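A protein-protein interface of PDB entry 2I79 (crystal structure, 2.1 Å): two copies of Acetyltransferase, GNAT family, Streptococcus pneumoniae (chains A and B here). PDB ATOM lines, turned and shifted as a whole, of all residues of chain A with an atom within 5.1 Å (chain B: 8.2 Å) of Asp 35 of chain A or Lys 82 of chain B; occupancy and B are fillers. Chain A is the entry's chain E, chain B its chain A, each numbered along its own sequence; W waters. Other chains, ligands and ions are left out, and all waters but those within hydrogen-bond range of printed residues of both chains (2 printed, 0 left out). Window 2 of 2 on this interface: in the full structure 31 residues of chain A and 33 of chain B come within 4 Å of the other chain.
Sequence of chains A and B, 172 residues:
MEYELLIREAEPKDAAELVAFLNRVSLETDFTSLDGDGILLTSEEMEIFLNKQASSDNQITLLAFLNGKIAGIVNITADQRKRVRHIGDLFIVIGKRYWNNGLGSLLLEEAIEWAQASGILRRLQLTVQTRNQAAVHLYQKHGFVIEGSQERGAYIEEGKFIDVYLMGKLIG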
ATOM      1  N   SER A  26     -22.344 -16.825   4.332  1.00  0.00           N
ATOM      2  CA  SER A  26     -20.946 -16.426   4.045  1.00  0.00           C
ATOM      3  C   SER A  26     -19.947 -16.985   5.054  1.00  0.00           C
ATOM      4  O   SER A  26     -18.774 -17.164   4.739  1.00  0.00           O
ATOM      5  CB  SER A  26     -20.824 -14.892   4.064  1.00  0.00           C
ATOM      6  OG  SER A  26     -21.539 -14.302   2.988  1.00  0.00           O
ATOM      7  N   LEU A  27     -20.416 -17.232   6.271  1.00  0.00           N
ATOM      8  CA  LEU A  27     -19.585 -17.749   7.339  1.00  0.00           C
ATOM      9  C   LEU A  27     -19.718 -19.264   7.500  1.00  0.00           C
ATOM     10  O   LEU A  27     -18.991 -19.842   8.297  1.00  0.00           O
ATOM     11  CB  LEU A  27     -19.971 -17.102   8.675  1.00  0.00           C
ATOM     12  CG  LEU A  27     -19.814 -15.586   8.828  1.00  0.00           C
ATOM     13  CD1 LEU A  27     -20.558 -15.147  10.060  1.00  0.00           C
ATOM     14  CD2 LEU A  27     -18.355 -15.208   8.908  1.00  0.00           C
ATOM     15  N   SER A  33     -17.826 -17.633  -3.649  1.00  0.00           N
ATOM     16  CA  SER A  33     -16.995 -16.430  -3.509  1.00  0.00           C
ATOM     17  C   SER A  33     -17.179 -15.681  -2.192  1.00  0.00           C
ATOM     18  O   SER A  33     -16.309 -14.881  -1.833  1.00  0.00           O
ATOM     19  CB  SER A  33     -17.283 -15.468  -4.643  1.00  0.00           C
ATOM     20  OG  SER A  33     -16.564 -15.880  -5.759  1.00  0.00           O
ATOM     21  N   LEU A  34     -18.292 -15.937  -1.499  1.00  0.00           N
ATOM     22  CA  LEU A  34     -18.553 -15.343  -0.201  1.00  0.00           C
ATOM     23  C   LEU A  34     -17.522 -15.849   0.783  1.00  0.00           C
ATOM     24  O   LEU A  34     -17.222 -17.044   0.816  1.00  0.00           O
ATOM     25  CB  LEU A  34     -19.958 -15.700   0.299  1.00  0.00           C
ATOM     26  CG  LEU A  34     -21.148 -15.137  -0.478  1.00  0.00           C
ATOM     27  CD1 LEU A  34     -22.441 -15.793   0.041  1.00  0.00           C
ATOM     28  CD2 LEU A  34     -21.195 -13.624  -0.333  1.00  0.00           C
ATOM     29  N   ASP A  35     -16.951 -14.931   1.541  1.00  0.00           N
ATOM     30  CA  ASP A  35     -16.059 -15.275   2.643  1.00  0.00           C
ATOM     31  C   ASP A  35     -16.494 -14.471   3.892  1.00  0.00           C
ATOM     32  O   ASP A  35     -17.567 -13.904   3.892  1.00  0.00           O
ATOM     33  CB  ASP A  35     -14.596 -15.034   2.269  1.00  0.00           C
ATOM     34  CG  ASP A  35     -14.317 -13.589   1.804  1.00  0.00           C
ATOM     35  OD1 ASP A  35     -15.053 -12.656   2.209  1.00  0.00           O
ATOM     36  OD2 ASP A  35     -13.347 -13.396   1.022  1.00  0.00           O
ATOM     37  N   GLY A  36     -15.679 -14.444   4.941  1.00  0.00           N
ATOM     38  CA  GLY A  36     -16.005 -13.711   6.181  1.00  0.00           C
ATOM     39  C   GLY A  36     -16.382 -12.239   6.042  1.00  0.00           C
ATOM     40  O   GLY A  36     -17.058 -11.689   6.924  1.00  0.00           O
ATOM     41  N   ASP A  37     -15.950 -11.591   4.963  1.00  0.00           N
ATOM     42  CA  ASP A  37     -16.330 -10.190   4.707  1.00  0.00           C
ATOM     43  C   ASP A  37     -17.814 -10.035   4.356  1.00  0.00           C
ATOM     44  O   ASP A  37     -18.326  -8.914   4.355  1.00  0.00           O
ATOM     45  CB  ASP A  37     -15.472  -9.546   3.603  1.00  0.00           C
ATOM     46  CG  ASP A  37     -14.042  -9.269   4.032  1.00  0.00           C
ATOM     47  OD1 ASP A  37     -13.590  -9.712   5.121  1.00  0.00           O
ATOM     48  OD2 ASP A  37     -13.339  -8.617   3.236  1.00  0.00           O
ATOM     49  N   GLY A  38     -18.503 -11.141   4.067  1.00  0.00           N
ATOM     50  CA  GLY A  38     -19.953 -11.110   3.832  1.00  0.00           C
ATOM     51  C   GLY A  38     -20.329 -10.572   2.472  1.00  0.00           C
ATOM     52  O   GLY A  38     -19.493 -10.524   1.554  1.00  0.00           O
ATOM     53  N   TYR A 155      -9.432 -19.635  -4.813  1.00  0.00           N
ATOM     54  CA  TYR A 155      -8.362 -19.527  -3.839  1.00  0.00           C
ATOM     55  C   TYR A 155      -9.027 -19.632  -2.484  1.00  0.00           C
ATOM     56  O   TYR A 155      -9.979 -18.946  -2.235  1.00  0.00           O
ATOM     57  CB  TYR A 155      -7.674 -18.188  -4.037  1.00  0.00           C
ATOM     58  CG  TYR A 155      -6.621 -17.813  -3.032  1.00  0.00           C
ATOM     59  CD1 TYR A 155      -5.316 -18.290  -3.150  1.00  0.00           C
ATOM     60  CD2 TYR A 155      -6.920 -16.946  -1.982  1.00  0.00           C
ATOM     61  CE1 TYR A 155      -4.337 -17.923  -2.246  1.00  0.00           C
ATOM     62  CE2 TYR A 155      -5.954 -16.577  -1.060  1.00  0.00           C
ATOM     63  CZ  TYR A 155      -4.657 -17.056  -1.210  1.00  0.00           C
ATOM     64  OH  TYR A 155      -3.685 -16.689  -0.293  1.00  0.00           O
ATOM     65  N   GLU A 158      -6.204 -18.971   2.648  1.00  0.00           N
ATOM     66  CA  GLU A 158      -5.038 -18.057   2.671  1.00  0.00           C
ATOM     67  C   GLU A 158      -3.778 -18.745   2.073  1.00  0.00           C
ATOM     68  O   GLU A 158      -2.812 -19.000   2.805  1.00  0.00           O
ATOM     69  CB  GLU A 158      -4.830 -17.585   4.138  1.00  0.00           C
ATOM     70  CG  GLU A 158      -3.717 -16.531   4.415  1.00  0.00           C
ATOM     71  CD  GLU A 158      -3.058 -16.733   5.806  1.00  0.00           C
ATOM     72  OE1 GLU A 158      -3.290 -15.876   6.704  1.00  0.00           O
ATOM     73  OE2 GLU A 158      -2.330 -17.758   5.996  1.00  0.00           O
ATOM     74  N   ASP B  79     -12.508  -9.342 -10.483  1.00  0.00           N
ATOM     75  CA  ASP B  79     -13.239  -9.159  -9.228  1.00  0.00           C
ATOM     76  C   ASP B  79     -12.304  -8.942  -8.066  1.00  0.00           C
ATOM     77  O   ASP B  79     -11.130  -9.256  -8.161  1.00  0.00           O
ATOM     78  CB  ASP B  79     -14.112 -10.381  -8.970  1.00  0.00           C
ATOM     79  CG  ASP B  79     -15.290 -10.444  -9.922  1.00  0.00           C
ATOM     80  OD1 ASP B  79     -15.515  -9.472 -10.694  1.00  0.00           O
ATOM     81  OD2 ASP B  79     -16.001 -11.458  -9.902  1.00  0.00           O
ATOM     82  N   GLN B  80     -12.834  -8.407  -6.963  1.00  0.00           N
ATOM     83  CA  GLN B  80     -12.007  -7.985  -5.836  1.00  0.00           C
ATOM     84  C   GLN B  80     -12.058  -8.905  -4.618  1.00  0.00           C
ATOM     85  O   GLN B  80     -11.193  -8.801  -3.758  1.00  0.00           O
ATOM     86  CB  GLN B  80     -12.360  -6.542  -5.418  1.00  0.00           C
ATOM     87  CG  GLN B  80     -12.043  -5.450  -6.458  1.00  0.00           C
ATOM     88  CD  GLN B  80     -10.648  -5.570  -7.036  1.00  0.00           C
ATOM     89  OE1 GLN B  80     -10.477  -5.695  -8.260  1.00  0.00           O
ATOM     90  NE2 GLN B  80      -9.648  -5.634  -6.160  1.00  0.00           N
ATOM     91  N   ARG B  81     -13.036  -9.805  -4.540  1.00  0.00           N
ATOM     92  CA  ARG B  81     -13.072 -10.831  -3.467  1.00  0.00           C
ATOM     93  C   ARG B  81     -11.900 -11.796  -3.536  1.00  0.00           C
ATOM     94  O   ARG B  81     -11.492 -12.218  -4.635  1.00  0.00           O
ATOM     95  CB  ARG B  81     -14.366 -11.628  -3.529  1.00  0.00           C
ATOM     96  CG  ARG B  81     -15.556 -10.850  -2.948  1.00  0.00           C
ATOM     97  CD  ARG B  81     -16.814 -11.674  -2.992  1.00  0.00           C
ATOM     98  NE  ARG B  81     -17.870 -11.145  -2.100  1.00  0.00           N
ATOM     99  CZ  ARG B  81     -18.853 -10.327  -2.485  1.00  0.00           C
ATOM    100  NH1 ARG B  81     -18.957  -9.908  -3.746  1.00  0.00           N
ATOM    101  NH2 ARG B  81     -19.754  -9.933  -1.596  1.00  0.00           N
ATOM    102  N   LYS B  82     -11.352 -12.157  -2.375  1.00  0.00           N
ATOM    103  CA  LYS B  82     -10.115 -12.939  -2.368  1.00  0.00           C
ATOM    104  C   LYS B  82     -10.241 -14.328  -2.987  1.00  0.00           C
ATOM    105  O   LYS B  82      -9.227 -14.876  -3.445  1.00  0.00           O
ATOM    106  CB  LYS B  82      -9.488 -13.021  -0.974  1.00  0.00           C
ATOM    107  CG  LYS B  82     -10.241 -13.852   0.032  1.00  0.00           C
ATOM    108  CD  LYS B  82      -9.666 -15.315   0.155  1.00  0.00           C
ATOM    109  CE  LYS B  82     -10.028 -15.976   1.506  1.00  0.00           C
ATOM    110  NZ  LYS B  82     -11.474 -15.748   1.901  1.00  0.00           N
ATOM    111  N   ARG B  83     -11.462 -14.885  -3.027  1.00  0.00           N
ATOM    112  CA  ARG B  83     -11.693 -16.166  -3.700  1.00  0.00           C
ATOM    113  C   ARG B  83     -11.170 -16.134  -5.144  1.00  0.00           C
ATOM    114  O   ARG B  83     -10.604 -17.108  -5.596  1.00  0.00           O
ATOM    115  CB  ARG B  83     -13.172 -16.572  -3.723  1.00  0.00           C
ATOM    116  CG  ARG B  83     -13.404 -18.097  -4.102  1.00  0.00           C
ATOM    117  CD  ARG B  83     -13.875 -18.957  -2.906  1.00  0.00           C
ATOM    118  NE  ARG B  83     -13.075 -18.669  -1.720  1.00  0.00           N
ATOM    119  CZ  ARG B  83     -13.497 -18.427  -0.498  1.00  0.00           C
ATOM    120  NH1 ARG B  83     -14.767 -18.458  -0.141  1.00  0.00           N
ATOM    121  NH2 ARG B  83     -12.580 -18.166   0.414  1.00  0.00           N
ATOM    122  N   VAL B  84     -11.350 -14.999  -5.830  1.00  0.00           N
ATOM    123  CA  VAL B  84     -11.147 -14.868  -7.278  1.00  0.00           C
ATOM    124  C   VAL B  84     -10.298 -13.663  -7.730  1.00  0.00           C
ATOM    125  O   VAL B  84     -10.119 -13.426  -8.928  1.00  0.00           O
ATOM    126  CB  VAL B  84     -12.516 -14.843  -7.987  1.00  0.00           C
ATOM    127  CG1 VAL B  84     -13.193 -16.190  -7.811  1.00  0.00           C
ATOM    128  CG2 VAL B  84     -13.385 -13.729  -7.458  1.00  0.00           C
ATOM    129  N   ARG B  85      -9.705 -12.962  -6.767  1.00  0.00           N
ATOM    130  CA  ARG B  85      -8.939 -11.717  -7.007  1.00  0.00           C
ATOM    131  C   ARG B  85      -7.687 -11.909  -7.914  1.00  0.00           C
ATOM    132  O   ARG B  85      -7.204 -10.964  -8.531  1.00  0.00           O
ATOM    133  CB  ARG B  85      -8.550 -11.132  -5.637  1.00  0.00           C
ATOM    134  CG  ARG B  85      -7.868  -9.800  -5.669  1.00  0.00           C
ATOM    135  CD  ARG B  85      -8.107  -9.005  -4.375  1.00  0.00           C
ATOM    136  NE  ARG B  85      -7.474  -9.631  -3.221  1.00  0.00           N
ATOM    137  CZ  ARG B  85      -7.928  -9.581  -1.960  1.00  0.00           C
ATOM    138  NH1 ARG B  85      -9.071  -8.968  -1.635  1.00  0.00           N
ATOM    139  NH2 ARG B  85      -7.228 -10.185  -0.996  1.00  0.00           N
ATOM    140  N   HIS B  86      -7.215 -13.142  -7.999  1.00  0.00           N
ATOM    141  CA  HIS B  86      -6.014 -13.532  -8.759  1.00  0.00           C
ATOM    142  C   HIS B  86      -6.293 -13.879 -10.223  1.00  0.00           C
ATOM    143  O   HIS B  86      -5.369 -14.220 -10.951  1.00  0.00           O
ATOM    144  CB  HIS B  86      -5.373 -14.756  -8.075  1.00  0.00           C
ATOM    145  CG  HIS B  86      -6.291 -15.938  -8.008  1.00  0.00           C
ATOM    146  ND1 HIS B  86      -6.230 -16.976  -8.915  1.00  0.00           N
ATOM    147  CD2 HIS B  86      -7.369 -16.186  -7.231  1.00  0.00           C
ATOM    148  CE1 HIS B  86      -7.190 -17.843  -8.645  1.00  0.00           C
ATOM    149  NE2 HIS B  86      -7.901 -17.379  -7.640  1.00  0.00           N
ATOM    150  N   ILE B  87      -7.558 -13.789 -10.637  1.00  0.00           N
ATOM    151  CA  ILE B  87      -8.011 -14.126 -11.980  1.00  0.00           C
ATOM    152  C   ILE B  87      -8.350 -12.857 -12.793  1.00  0.00           C
ATOM    153  O   ILE B  87      -9.253 -12.090 -12.428  1.00  0.00           O
ATOM    154  CB  ILE B  87      -9.293 -14.996 -11.926  1.00  0.00           C
ATOM    155  CG1 ILE B  87      -9.078 -16.266 -11.075  1.00  0.00           C
ATOM    156  CG2 ILE B  87      -9.757 -15.368 -13.329  1.00  0.00           C
ATOM    157  CD1 ILE B  87     -10.361 -17.006 -10.746  1.00  0.00           C
ATOM    158  N   ILE B 120      -0.420 -10.152  -7.965  1.00  0.00           N
ATOM    159  CA  ILE B 120      -1.788 -10.484  -7.543  1.00  0.00           C
ATOM    160  C   ILE B 120      -2.394 -11.491  -8.523  1.00  0.00           C
ATOM    161  O   ILE B 120      -2.965 -12.499  -8.116  1.00  0.00           O
ATOM    162  CB  ILE B 120      -2.676  -9.227  -7.465  1.00  0.00           C
ATOM    163  CG1 ILE B 120      -1.984  -8.133  -6.629  1.00  0.00           C
ATOM    164  CG2 ILE B 120      -4.076  -9.561  -6.864  1.00  0.00           C
ATOM    165  CD1 ILE B 120      -2.561  -6.711  -6.793  1.00  0.00           C
HETATM  166  O   HOH W   1     -17.419 -11.992   0.695  1.00  0.00           O
HETATM  167  O   HOH W   2     -13.809 -14.411  -1.416  1.00  0.00           O
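The side-chain carboxylate (OD2) of Asp 35 of chain A lies within salt-bridge range of the side-chain amino group (NZ) of Lys 82 of chain B.
O of Arg 83 of chain B is in hydrogen-bond range of N of Tyr 155 of chain A (2.9 Å).
NH2 of Arg 81 of chain B lies within hydrogen-bond range of O of Gly 38 of chain A, at 3.2 Å.
NH1 of Arg 83 of chain B is in hydrogen-bond range of O of Leu 34 of chain A, at 3.0 Å.
A ring nitrogen (NE2) of His 86 of chain B sits at hydrogen-bond distance from the backbone carbonyl oxygen (O) of Arg 83 of chain B, at 3.4 Å.
N of Asp 37 of chain A lies within hydrogen-bond range of OD1 of Asp 35 of chain A (3.1 Å).
Ser 33 of chain A touches Arg 81 of chain B (O to CD, 3.4 Å).
Arg 83 of chain B touches Ser 33 of chain A.
OG of Ser 33 of chain A touches CG1 of Val 84 of chain B, 3.96 Å away.
CD2 of Tyr 155 of chain A touches O of Lys 82 of chain B, 3.4 Å away.
NE2 of His 86 of chain B touches CB of Tyr 155 of chain A, 3.7 Å away.
Of the printed residues of chain B, Asp 35 of chain A touches Lys 82 (3.1 Å).
Lys 82 of chain B touches two residues of chain A.
No residue of chain B comes within 4 Å of Gly 36 of chain A.
Of the printed residues of chain A, Arg 81 of chain B touches Ser 33 and Gly 38.
Of the printed residues of chain A, Val 84 of chain B touches Ser 33.
Of the printed residues of chain B, Ser 33 of chain A touches Arg 81, Arg 83 and Val 84.
Glu 158 of chain A touches none of the printed residues of chain B.
Gln 80 of chain B touches none of the printed residues of chain A.
The nearest residue of chain A that does not touch Lys 82 of chain B is Glu 158 of chain A (5.0 Å).
Of the 10 printed residues of chain A, 5 touch a printed residue of chain B.
Hydrophobic or aromatic side chains of chain A that line the printed part of chain B: Tyr 155.
Among the printed residues, 9 pairs touch across the chains.
Among the printed residues, Asp or Glu carboxylates within 4 Å of a Lys or Arg side-chain nitrogen of the other chain: Asp 35 of chain A with Lys 82 of chain B (3.1 Å).
No position is printed for both chains.
Water W2 lies within hydrogen-bond range of O of Ser 33 of chain A (2.6 Å), OD2 of Asp 35 of chain A (2.7 Å), N of Arg 83 of chain B (2.9 Å) and N of Lys 82 of chain B (3.5 Å).
Water W1 lies within hydrogen-bond range of the backbone carbonyl oxygen of Gly 38 of chain A (2.7 Å), the side-chain carboxylate of Asp 35 of chain A (2.9 Å) and the guanidinium group of Arg 81 of chain B (3.0 Å).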
